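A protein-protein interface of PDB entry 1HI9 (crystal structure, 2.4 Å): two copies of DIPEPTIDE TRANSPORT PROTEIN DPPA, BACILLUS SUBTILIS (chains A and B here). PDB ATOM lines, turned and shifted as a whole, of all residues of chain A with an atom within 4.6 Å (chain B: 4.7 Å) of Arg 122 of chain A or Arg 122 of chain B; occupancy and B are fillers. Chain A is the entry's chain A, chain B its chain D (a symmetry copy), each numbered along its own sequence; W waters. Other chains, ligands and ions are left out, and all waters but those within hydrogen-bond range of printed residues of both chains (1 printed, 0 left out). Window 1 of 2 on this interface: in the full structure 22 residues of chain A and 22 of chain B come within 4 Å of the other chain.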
ATOM      1  N   ALA A 107       3.677  -4.915   9.566  1.00  0.00           N
ATOM      2  CA  ALA A 107       4.381  -6.117   9.121  1.00  0.00           C
ATOM      3  C   ALA A 107       4.341  -6.342   7.614  1.00  0.00           C
ATOM      4  O   ALA A 107       3.411  -5.909   6.936  1.00  0.00           O
ATOM      5  CB  ALA A 107       3.800  -7.335   9.828  1.00  0.00           C
ATOM      6  N   SER A 108       5.370  -7.007   7.103  1.00  0.00           N
ATOM      7  CA  SER A 108       5.454  -7.346   5.694  1.00  0.00           C
ATOM      8  C   SER A 108       5.677  -6.178   4.732  1.00  0.00           C
ATOM      9  O   SER A 108       5.551  -6.350   3.526  1.00  0.00           O
ATOM     10  CB  SER A 108       4.186  -8.112   5.292  1.00  0.00           C
ATOM     11  OG  SER A 108       3.973  -9.219   6.153  1.00  0.00           O
ATOM     12  N   GLY A 120       4.907 -12.874  14.856  1.00  0.00           N
ATOM     13  CA  GLY A 120       4.105 -13.821  14.109  1.00  0.00           C
ATOM     14  C   GLY A 120       3.035 -13.334  13.144  1.00  0.00           C
ATOM     15  O   GLY A 120       2.551 -14.123  12.331  1.00  0.00           O
ATOM     16  N   VAL A 121       2.640 -12.068  13.200  1.00  0.00           N
ATOM     17  CA  VAL A 121       1.599 -11.640  12.278  1.00  0.00           C
ATOM     18  C   VAL A 121       2.157 -11.037  11.002  1.00  0.00           C
ATOM     19  O   VAL A 121       3.166 -10.318  11.015  1.00  0.00           O
ATOM     20  CB  VAL A 121       0.621 -10.611  12.899  1.00  0.00           C
ATOM     21  CG1 VAL A 121       0.205 -11.045  14.291  1.00  0.00           C
ATOM     22  CG2 VAL A 121       1.246  -9.241  12.911  1.00  0.00           C
ATOM     23  N   ARG A 122       1.507 -11.348   9.888  1.00  0.00           N
ATOM     24  CA  ARG A 122       1.927 -10.801   8.607  1.00  0.00           C
ATOM     25  C   ARG A 122       1.038  -9.637   8.232  1.00  0.00           C
ATOM     26  O   ARG A 122       1.522  -8.643   7.703  1.00  0.00           O
ATOM     27  CB  ARG A 122       1.878 -11.869   7.519  1.00  0.00           C
ATOM     28  CG  ARG A 122       3.179 -12.627   7.373  1.00  0.00           C
ATOM     29  CD  ARG A 122       3.052 -13.646   6.289  1.00  0.00           C
ATOM     30  NE  ARG A 122       2.680 -13.068   4.991  1.00  0.00           N
ATOM     31  CZ  ARG A 122       3.526 -12.462   4.166  1.00  0.00           C
ATOM     32  NH1 ARG A 122       4.806 -12.340   4.494  1.00  0.00           N
ATOM     33  NH2 ARG A 122       3.102 -12.002   3.002  1.00  0.00           N
ATOM     34  N   HIS A 123      -0.258  -9.765   8.511  1.00  0.00           N
ATOM     35  CA  HIS A 123      -1.217  -8.704   8.212  1.00  0.00           C
ATOM     36  C   HIS A 123      -2.412  -8.708   9.163  1.00  0.00           C
ATOM     37  O   HIS A 123      -2.838  -9.753   9.655  1.00  0.00           O
ATOM     38  CB  HIS A 123      -1.779  -8.837   6.784  1.00  0.00           C
ATOM     39  CG  HIS A 123      -0.775  -8.605   5.698  1.00  0.00           C
ATOM     40  ND1 HIS A 123      -0.317  -9.613   4.880  1.00  0.00           N
ATOM     41  CD2 HIS A 123      -0.130  -7.480   5.307  1.00  0.00           C
ATOM     42  CE1 HIS A 123       0.572  -9.125   4.033  1.00  0.00           C
ATOM     43  NE2 HIS A 123       0.703  -7.831   4.271  1.00  0.00           N
ATOM     44  N   GLU A 222      -3.508 -12.613   9.447  1.00  0.00           N
ATOM     45  CA  GLU A 222      -2.753 -13.584   8.679  1.00  0.00           C
ATOM     46  C   GLU A 222      -1.450 -13.795   9.443  1.00  0.00           C
ATOM     47  O   GLU A 222      -0.692 -12.846   9.657  1.00  0.00           O
ATOM     48  CB  GLU A 222      -2.454 -13.047   7.288  1.00  0.00           C
ATOM     49  CG  GLU A 222      -1.796 -14.069   6.384  1.00  0.00           C
ATOM     50  CD  GLU A 222      -1.452 -13.500   5.017  1.00  0.00           C
ATOM     51  OE1 GLU A 222      -2.354 -12.961   4.343  1.00  0.00           O
ATOM     52  OE2 GLU A 222      -0.276 -13.595   4.623  1.00  0.00           O
ATOM     53  N   PHE A 223      -1.196 -15.031   9.862  1.00  0.00           N
ATOM     54  CA  PHE A 223       0.017 -15.354  10.606  1.00  0.00           C
ATOM     55  C   PHE A 223       1.113 -15.893   9.692  1.00  0.00           C
ATOM     56  O   PHE A 223       0.851 -16.306   8.559  1.00  0.00           O
ATOM     57  CB  PHE A 223      -0.302 -16.376  11.705  1.00  0.00           C
ATOM     58  CG  PHE A 223      -1.266 -15.865  12.738  1.00  0.00           C
ATOM     59  CD1 PHE A 223      -2.629 -16.129  12.630  1.00  0.00           C
ATOM     60  CD2 PHE A 223      -0.813 -15.090  13.809  1.00  0.00           C
ATOM     61  CE1 PHE A 223      -3.534 -15.627  13.572  1.00  0.00           C
ATOM     62  CE2 PHE A 223      -1.706 -14.577  14.761  1.00  0.00           C
ATOM     63  CZ  PHE A 223      -3.075 -14.845  14.645  1.00  0.00           C
ATOM     64  N   ALA A 224       2.345 -15.889  10.190  1.00  0.00           N
ATOM     65  CA  ALA A 224       3.481 -16.363   9.409  1.00  0.00           C
ATOM     66  C   ALA A 224       3.401 -17.851   9.075  1.00  0.00           C
ATOM     67  O   ALA A 224       3.717 -18.243   7.949  1.00  0.00           O
ATOM     68  CB  ALA A 224       4.778 -16.060  10.145  1.00  0.00           C
ATOM     69  N   THR A 245      -3.311 -19.080   6.250  1.00  0.00           N
ATOM     70  CA  THR A 245      -2.862 -19.064   7.631  1.00  0.00           C
ATOM     71  C   THR A 245      -3.557 -17.882   8.284  1.00  0.00           C
ATOM     72  O   THR A 245      -3.071 -17.303   9.262  1.00  0.00           O
ATOM     73  CB  THR A 245      -1.349 -18.861   7.730  1.00  0.00           C
ATOM     74  OG1 THR A 245      -1.002 -17.610   7.125  1.00  0.00           O
ATOM     75  CG2 THR A 245      -0.618 -19.994   7.031  1.00  0.00           C
ATOM     76  N   ALA B 107       5.627 -24.951   3.896  1.00  0.00           N
ATOM     77  CA  ALA B 107       5.278 -23.837   4.774  1.00  0.00           C
ATOM     78  C   ALA B 107       3.901 -23.248   4.505  1.00  0.00           C
ATOM     79  O   ALA B 107       3.405 -23.290   3.379  1.00  0.00           O
ATOM     80  CB  ALA B 107       6.328 -22.739   4.648  1.00  0.00           C
ATOM     81  N   SER B 108       3.288 -22.714   5.555  1.00  0.00           N
ATOM     82  CA  SER B 108       2.001 -22.061   5.438  1.00  0.00           C
ATOM     83  C   SER B 108       0.798 -22.981   5.185  1.00  0.00           C
ATOM     84  O   SER B 108      -0.288 -22.510   4.849  1.00  0.00           O
ATOM     85  CB  SER B 108       2.091 -21.008   4.333  1.00  0.00           C
ATOM     86  OG  SER B 108       3.199 -20.143   4.557  1.00  0.00           O
ATOM     87  N   GLY B 120      11.925 -18.963   8.037  1.00  0.00           N
ATOM     88  CA  GLY B 120      11.600 -17.720   7.365  1.00  0.00           C
ATOM     89  C   GLY B 120      10.873 -17.742   6.038  1.00  0.00           C
ATOM     90  O   GLY B 120      10.388 -16.696   5.610  1.00  0.00           O
ATOM     91  N   VAL B 121      10.799 -18.884   5.359  1.00  0.00           N
ATOM     92  CA  VAL B 121      10.081 -18.886   4.087  1.00  0.00           C
ATOM     93  C   VAL B 121       8.611 -19.254   4.253  1.00  0.00           C
ATOM     94  O   VAL B 121       8.262 -20.105   5.063  1.00  0.00           O
ATOM     95  CB  VAL B 121      10.697 -19.851   3.044  1.00  0.00           C
ATOM     96  CG1 VAL B 121      12.188 -19.711   3.011  1.00  0.00           C
ATOM     97  CG2 VAL B 121      10.286 -21.244   3.328  1.00  0.00           C
ATOM     98  N   ARG B 122       7.759 -18.579   3.490  1.00  0.00           N
ATOM     99  CA  ARG B 122       6.334 -18.844   3.512  1.00  0.00           C
ATOM    100  C   ARG B 122       5.956 -19.669   2.295  1.00  0.00           C
ATOM    101  O   ARG B 122       5.127 -20.564   2.393  1.00  0.00           O
ATOM    102  CB  ARG B 122       5.542 -17.547   3.508  1.00  0.00           C
ATOM    103  CG  ARG B 122       5.186 -17.049   4.887  1.00  0.00           C
ATOM    104  CD  ARG B 122       4.409 -15.772   4.763  1.00  0.00           C
ATOM    105  NE  ARG B 122       3.151 -15.938   4.037  1.00  0.00           N
ATOM    106  CZ  ARG B 122       2.046 -16.472   4.552  1.00  0.00           C
ATOM    107  NH1 ARG B 122       2.030 -16.907   5.803  1.00  0.00           N
ATOM    108  NH2 ARG B 122       0.946 -16.540   3.823  1.00  0.00           N
ATOM    109  N   HIS B 123       6.565 -19.360   1.154  1.00  0.00           N
ATOM    110  CA  HIS B 123       6.294 -20.087  -0.081  1.00  0.00           C
ATOM    111  C   HIS B 123       7.470 -20.104  -1.046  1.00  0.00           C
ATOM    112  O   HIS B 123       8.231 -19.141  -1.131  1.00  0.00           O
ATOM    113  CB  HIS B 123       5.106 -19.476  -0.827  1.00  0.00           C
ATOM    114  CG  HIS B 123       3.795 -19.646  -0.135  1.00  0.00           C
ATOM    115  ND1 HIS B 123       3.083 -18.581   0.375  1.00  0.00           N
ATOM    116  CD2 HIS B 123       3.061 -20.753   0.127  1.00  0.00           C
ATOM    117  CE1 HIS B 123       1.967 -19.027   0.923  1.00  0.00           C
ATOM    118  NE2 HIS B 123       1.931 -20.341   0.787  1.00  0.00           N
ATOM    119  N   PHE B 124       7.604 -21.212  -1.764  1.00  0.00           N
ATOM    120  CA  PHE B 124       8.619 -21.385  -2.795  1.00  0.00           C
ATOM    121  C   PHE B 124       7.821 -21.432  -4.099  1.00  0.00           C
ATOM    122  O   PHE B 124       6.733 -22.012  -4.140  1.00  0.00           O
ATOM    123  CB  PHE B 124       9.355 -22.718  -2.625  1.00  0.00           C
ATOM    124  CG  PHE B 124      10.535 -22.661  -1.698  1.00  0.00           C
ATOM    125  CD1 PHE B 124      11.014 -23.818  -1.096  1.00  0.00           C
ATOM    126  CD2 PHE B 124      11.175 -21.463  -1.432  1.00  0.00           C
ATOM    127  CE1 PHE B 124      12.110 -23.775  -0.239  1.00  0.00           C
ATOM    128  CE2 PHE B 124      12.264 -21.421  -0.582  1.00  0.00           C
ATOM    129  CZ  PHE B 124      12.731 -22.580   0.014  1.00  0.00           C
ATOM    130  N   GLU B 222       8.795 -16.263  -1.069  1.00  0.00           N
ATOM    131  CA  GLU B 222       8.079 -15.292  -0.265  1.00  0.00           C
ATOM    132  C   GLU B 222       8.538 -15.535   1.170  1.00  0.00           C
ATOM    133  O   GLU B 222       8.410 -16.645   1.697  1.00  0.00           O
ATOM    134  CB  GLU B 222       6.569 -15.503  -0.380  1.00  0.00           C
ATOM    135  CG  GLU B 222       5.750 -14.427   0.316  1.00  0.00           C
ATOM    136  CD  GLU B 222       4.262 -14.680   0.227  1.00  0.00           C
ATOM    137  OE1 GLU B 222       3.744 -14.851  -0.903  1.00  0.00           O
ATOM    138  OE2 GLU B 222       3.600 -14.711   1.287  1.00  0.00           O
ATOM    139  N   PHE B 223       9.094 -14.505   1.793  1.00  0.00           N
ATOM    140  CA  PHE B 223       9.579 -14.614   3.164  1.00  0.00           C
ATOM    141  C   PHE B 223       8.574 -14.079   4.173  1.00  0.00           C
ATOM    142  O   PHE B 223       7.668 -13.326   3.824  1.00  0.00           O
ATOM    143  CB  PHE B 223      10.916 -13.872   3.319  1.00  0.00           C
ATOM    144  CG  PHE B 223      12.025 -14.436   2.477  1.00  0.00           C
ATOM    145  CD1 PHE B 223      12.303 -13.906   1.223  1.00  0.00           C
ATOM    146  CD2 PHE B 223      12.787 -15.506   2.939  1.00  0.00           C
ATOM    147  CE1 PHE B 223      13.319 -14.437   0.434  1.00  0.00           C
ATOM    148  CE2 PHE B 223      13.805 -16.049   2.160  1.00  0.00           C
ATOM    149  CZ  PHE B 223      14.075 -15.510   0.908  1.00  0.00           C
ATOM    150  N   ALA B 224       8.731 -14.473   5.430  1.00  0.00           N
ATOM    151  CA  ALA B 224       7.819 -14.030   6.478  1.00  0.00           C
ATOM    152  C   ALA B 224       7.808 -12.515   6.675  1.00  0.00           C
ATOM    153  O   ALA B 224       6.738 -11.927   6.809  1.00  0.00           O
ATOM    154  CB  ALA B 224       8.156 -14.733   7.797  1.00  0.00           C
ATOM    155  N   THR B 245       6.984  -9.370   0.062  1.00  0.00           N
ATOM    156  CA  THR B 245       8.190  -9.807   0.753  1.00  0.00           C
ATOM    157  C   THR B 245       8.751 -10.964  -0.067  1.00  0.00           C
ATOM    158  O   THR B 245       9.450 -11.838   0.440  1.00  0.00           O
ATOM    159  CB  THR B 245       7.878 -10.294   2.182  1.00  0.00           C
ATOM    160  OG1 THR B 245       6.984 -11.418   2.134  1.00  0.00           O
ATOM    161  CG2 THR B 245       7.248  -9.174   2.990  1.00  0.00           C
HETATM  162  O   HOH W   1       5.628  -9.894   8.251  1.00  0.00           O
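Water W1 lies within hydrogen-bond range of O of Ala 224 of chain B and OG of Ser 108 of chain A.
Among the printed residues, merely in contact across the chains: Ser 108 of chain A with Thr 245 of chain B (3.3 Å), Thr 245 of chain A with Ser 108 of chain B (3.3 Å), Ala 224 of chain A with Ser 108 of chain B (3.9 Å) and Ser 108 of chain A with Ala 224 of chain B (3.9 Å).
Of the 10 printed residues of chain A, 6 touch a printed residue of chain B.
Of the 11 printed residues of chain B, 6 touch a printed residue of chain A.
Among the printed residues, Asp or Glu carboxylates within 4 Å of a Lys or Arg side-chain nitrogen of the other chain: Arg 122 of chain A with Glu 222 of chain B (3.2 Å) and Glu 222 of chain A with Arg 122 of chain B (3.3 Å).
Arg 122 of chain A touches five residues of chain B.
Of the printed residues of chain A, Arg 122 of chain B touches Arg 122 (2.9 Å), Glu 222 (3.3 Å), Phe 223 (3.1 Å), Ala 224 (3.0 Å) and Thr 245 (3.4 Å).
Of the printed residues of chain B, Thr 245 of chain A touches Ser 108 and Arg 122.
Of the printed residues of chain A, Glu 222 of chain B touches Arg 122.
Of the printed residues of chain A, Ser 108 of chain B touches Ala 224 and Thr 245.
Val 121 of chain A touches none of the printed residues of chain B.
The nearest printed residue of chain A that does not touch Ala 224 of chain B is Ala 224 of chain A (4.3 Å).
N of Glu 222 of chain A lies within hydrogen-bond range of O of His 123 of chain A (2.9 Å).
The backbone carbonyl oxygen of Phe 223 of chain A is in hydrogen-bond range of the side-chain hydroxyl of Thr 245 of chain A (2.7 Å).
The backbone NH (N) of Ala 224 of chain A sits at hydrogen-bond distance from the backbone carbonyl oxygen (O) of Gly 120 of chain A, at 2.8 Å.
NE of Arg 122 of chain B lies within salt-bridge range of OE2 of Glu 222 of chain B (3.0 Å).
The backbone carbonyl oxygen (O) of His 123 of chain B is in hydrogen-bond range of the backbone NH (N) of Glu 222 of chain B, 2.9 Å away.
The side-chain hydroxyl of Ser 108 of chain B sits at hydrogen-bond distance from the backbone carbonyl oxygen of Arg 122 of chain B, at 2.9 Å.
Arg 122 of chain A touches its own counterpart, Arg 122 of chain B.
Arg 122 of chain A touches Glu 222 of chain B, and with the chains exchanged Glu 222 of chain A touches Arg 122 of chain B.
Arg 122 of chain A touches Phe 223 of chain B, and with the chains exchanged Phe 223 of chain A touches Arg 122 of chain B.
Arg 122 of chain A touches Thr 245 of chain B, and with the chains exchanged Thr 245 of chain A touches Arg 122 of chain B.
10 positions are printed for both chains.
The side-chain carboxylate (OE2) of Glu 222 of chain B is in salt-bridge range of the guanidinium group (NH2) of Arg 122 of chain A (3.2 Å).
The backbone carbonyl oxygen of Ala 224 of chain B lies within hydrogen-bond range of the guanidinium group of Arg 122 of chain A (3.0 Å).
The guanidinium group (NH1) of Arg 122 of chain A sits at hydrogen-bond distance from the backbone carbonyl oxygen (O) of Phe 223 of chain B (3.1 Å).
The guanidinium group (NH1) of Arg 122 of chain A is in hydrogen-bond range of the side-chain hydroxyl (OG1) of Thr 245 of chain B (3.3 Å).
The backbone carbonyl oxygen of Phe 223 of chain A is in hydrogen-bond range of the guanidinium group of Arg 122 of chain B, 3.1 Å away.
The side-chain hydroxyl (OG1) of Thr 245 of chain A is in hydrogen-bond range of the guanidinium group (NH1) of Arg 122 of chain B (3.4 Å).
OE2 of Glu 222 of chain A is in salt-bridge range of NH2 of Arg 122 of chain B (3.3 Å).
The guanidinium group (NH1) of Arg 122 of chain B lies within hydrogen-bond range of the backbone carbonyl oxygen (O) of Ala 224 of chain A.
NE of Arg 122 of chain A sits close to NE of Arg 122 of chain B, at 3.1 Å.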
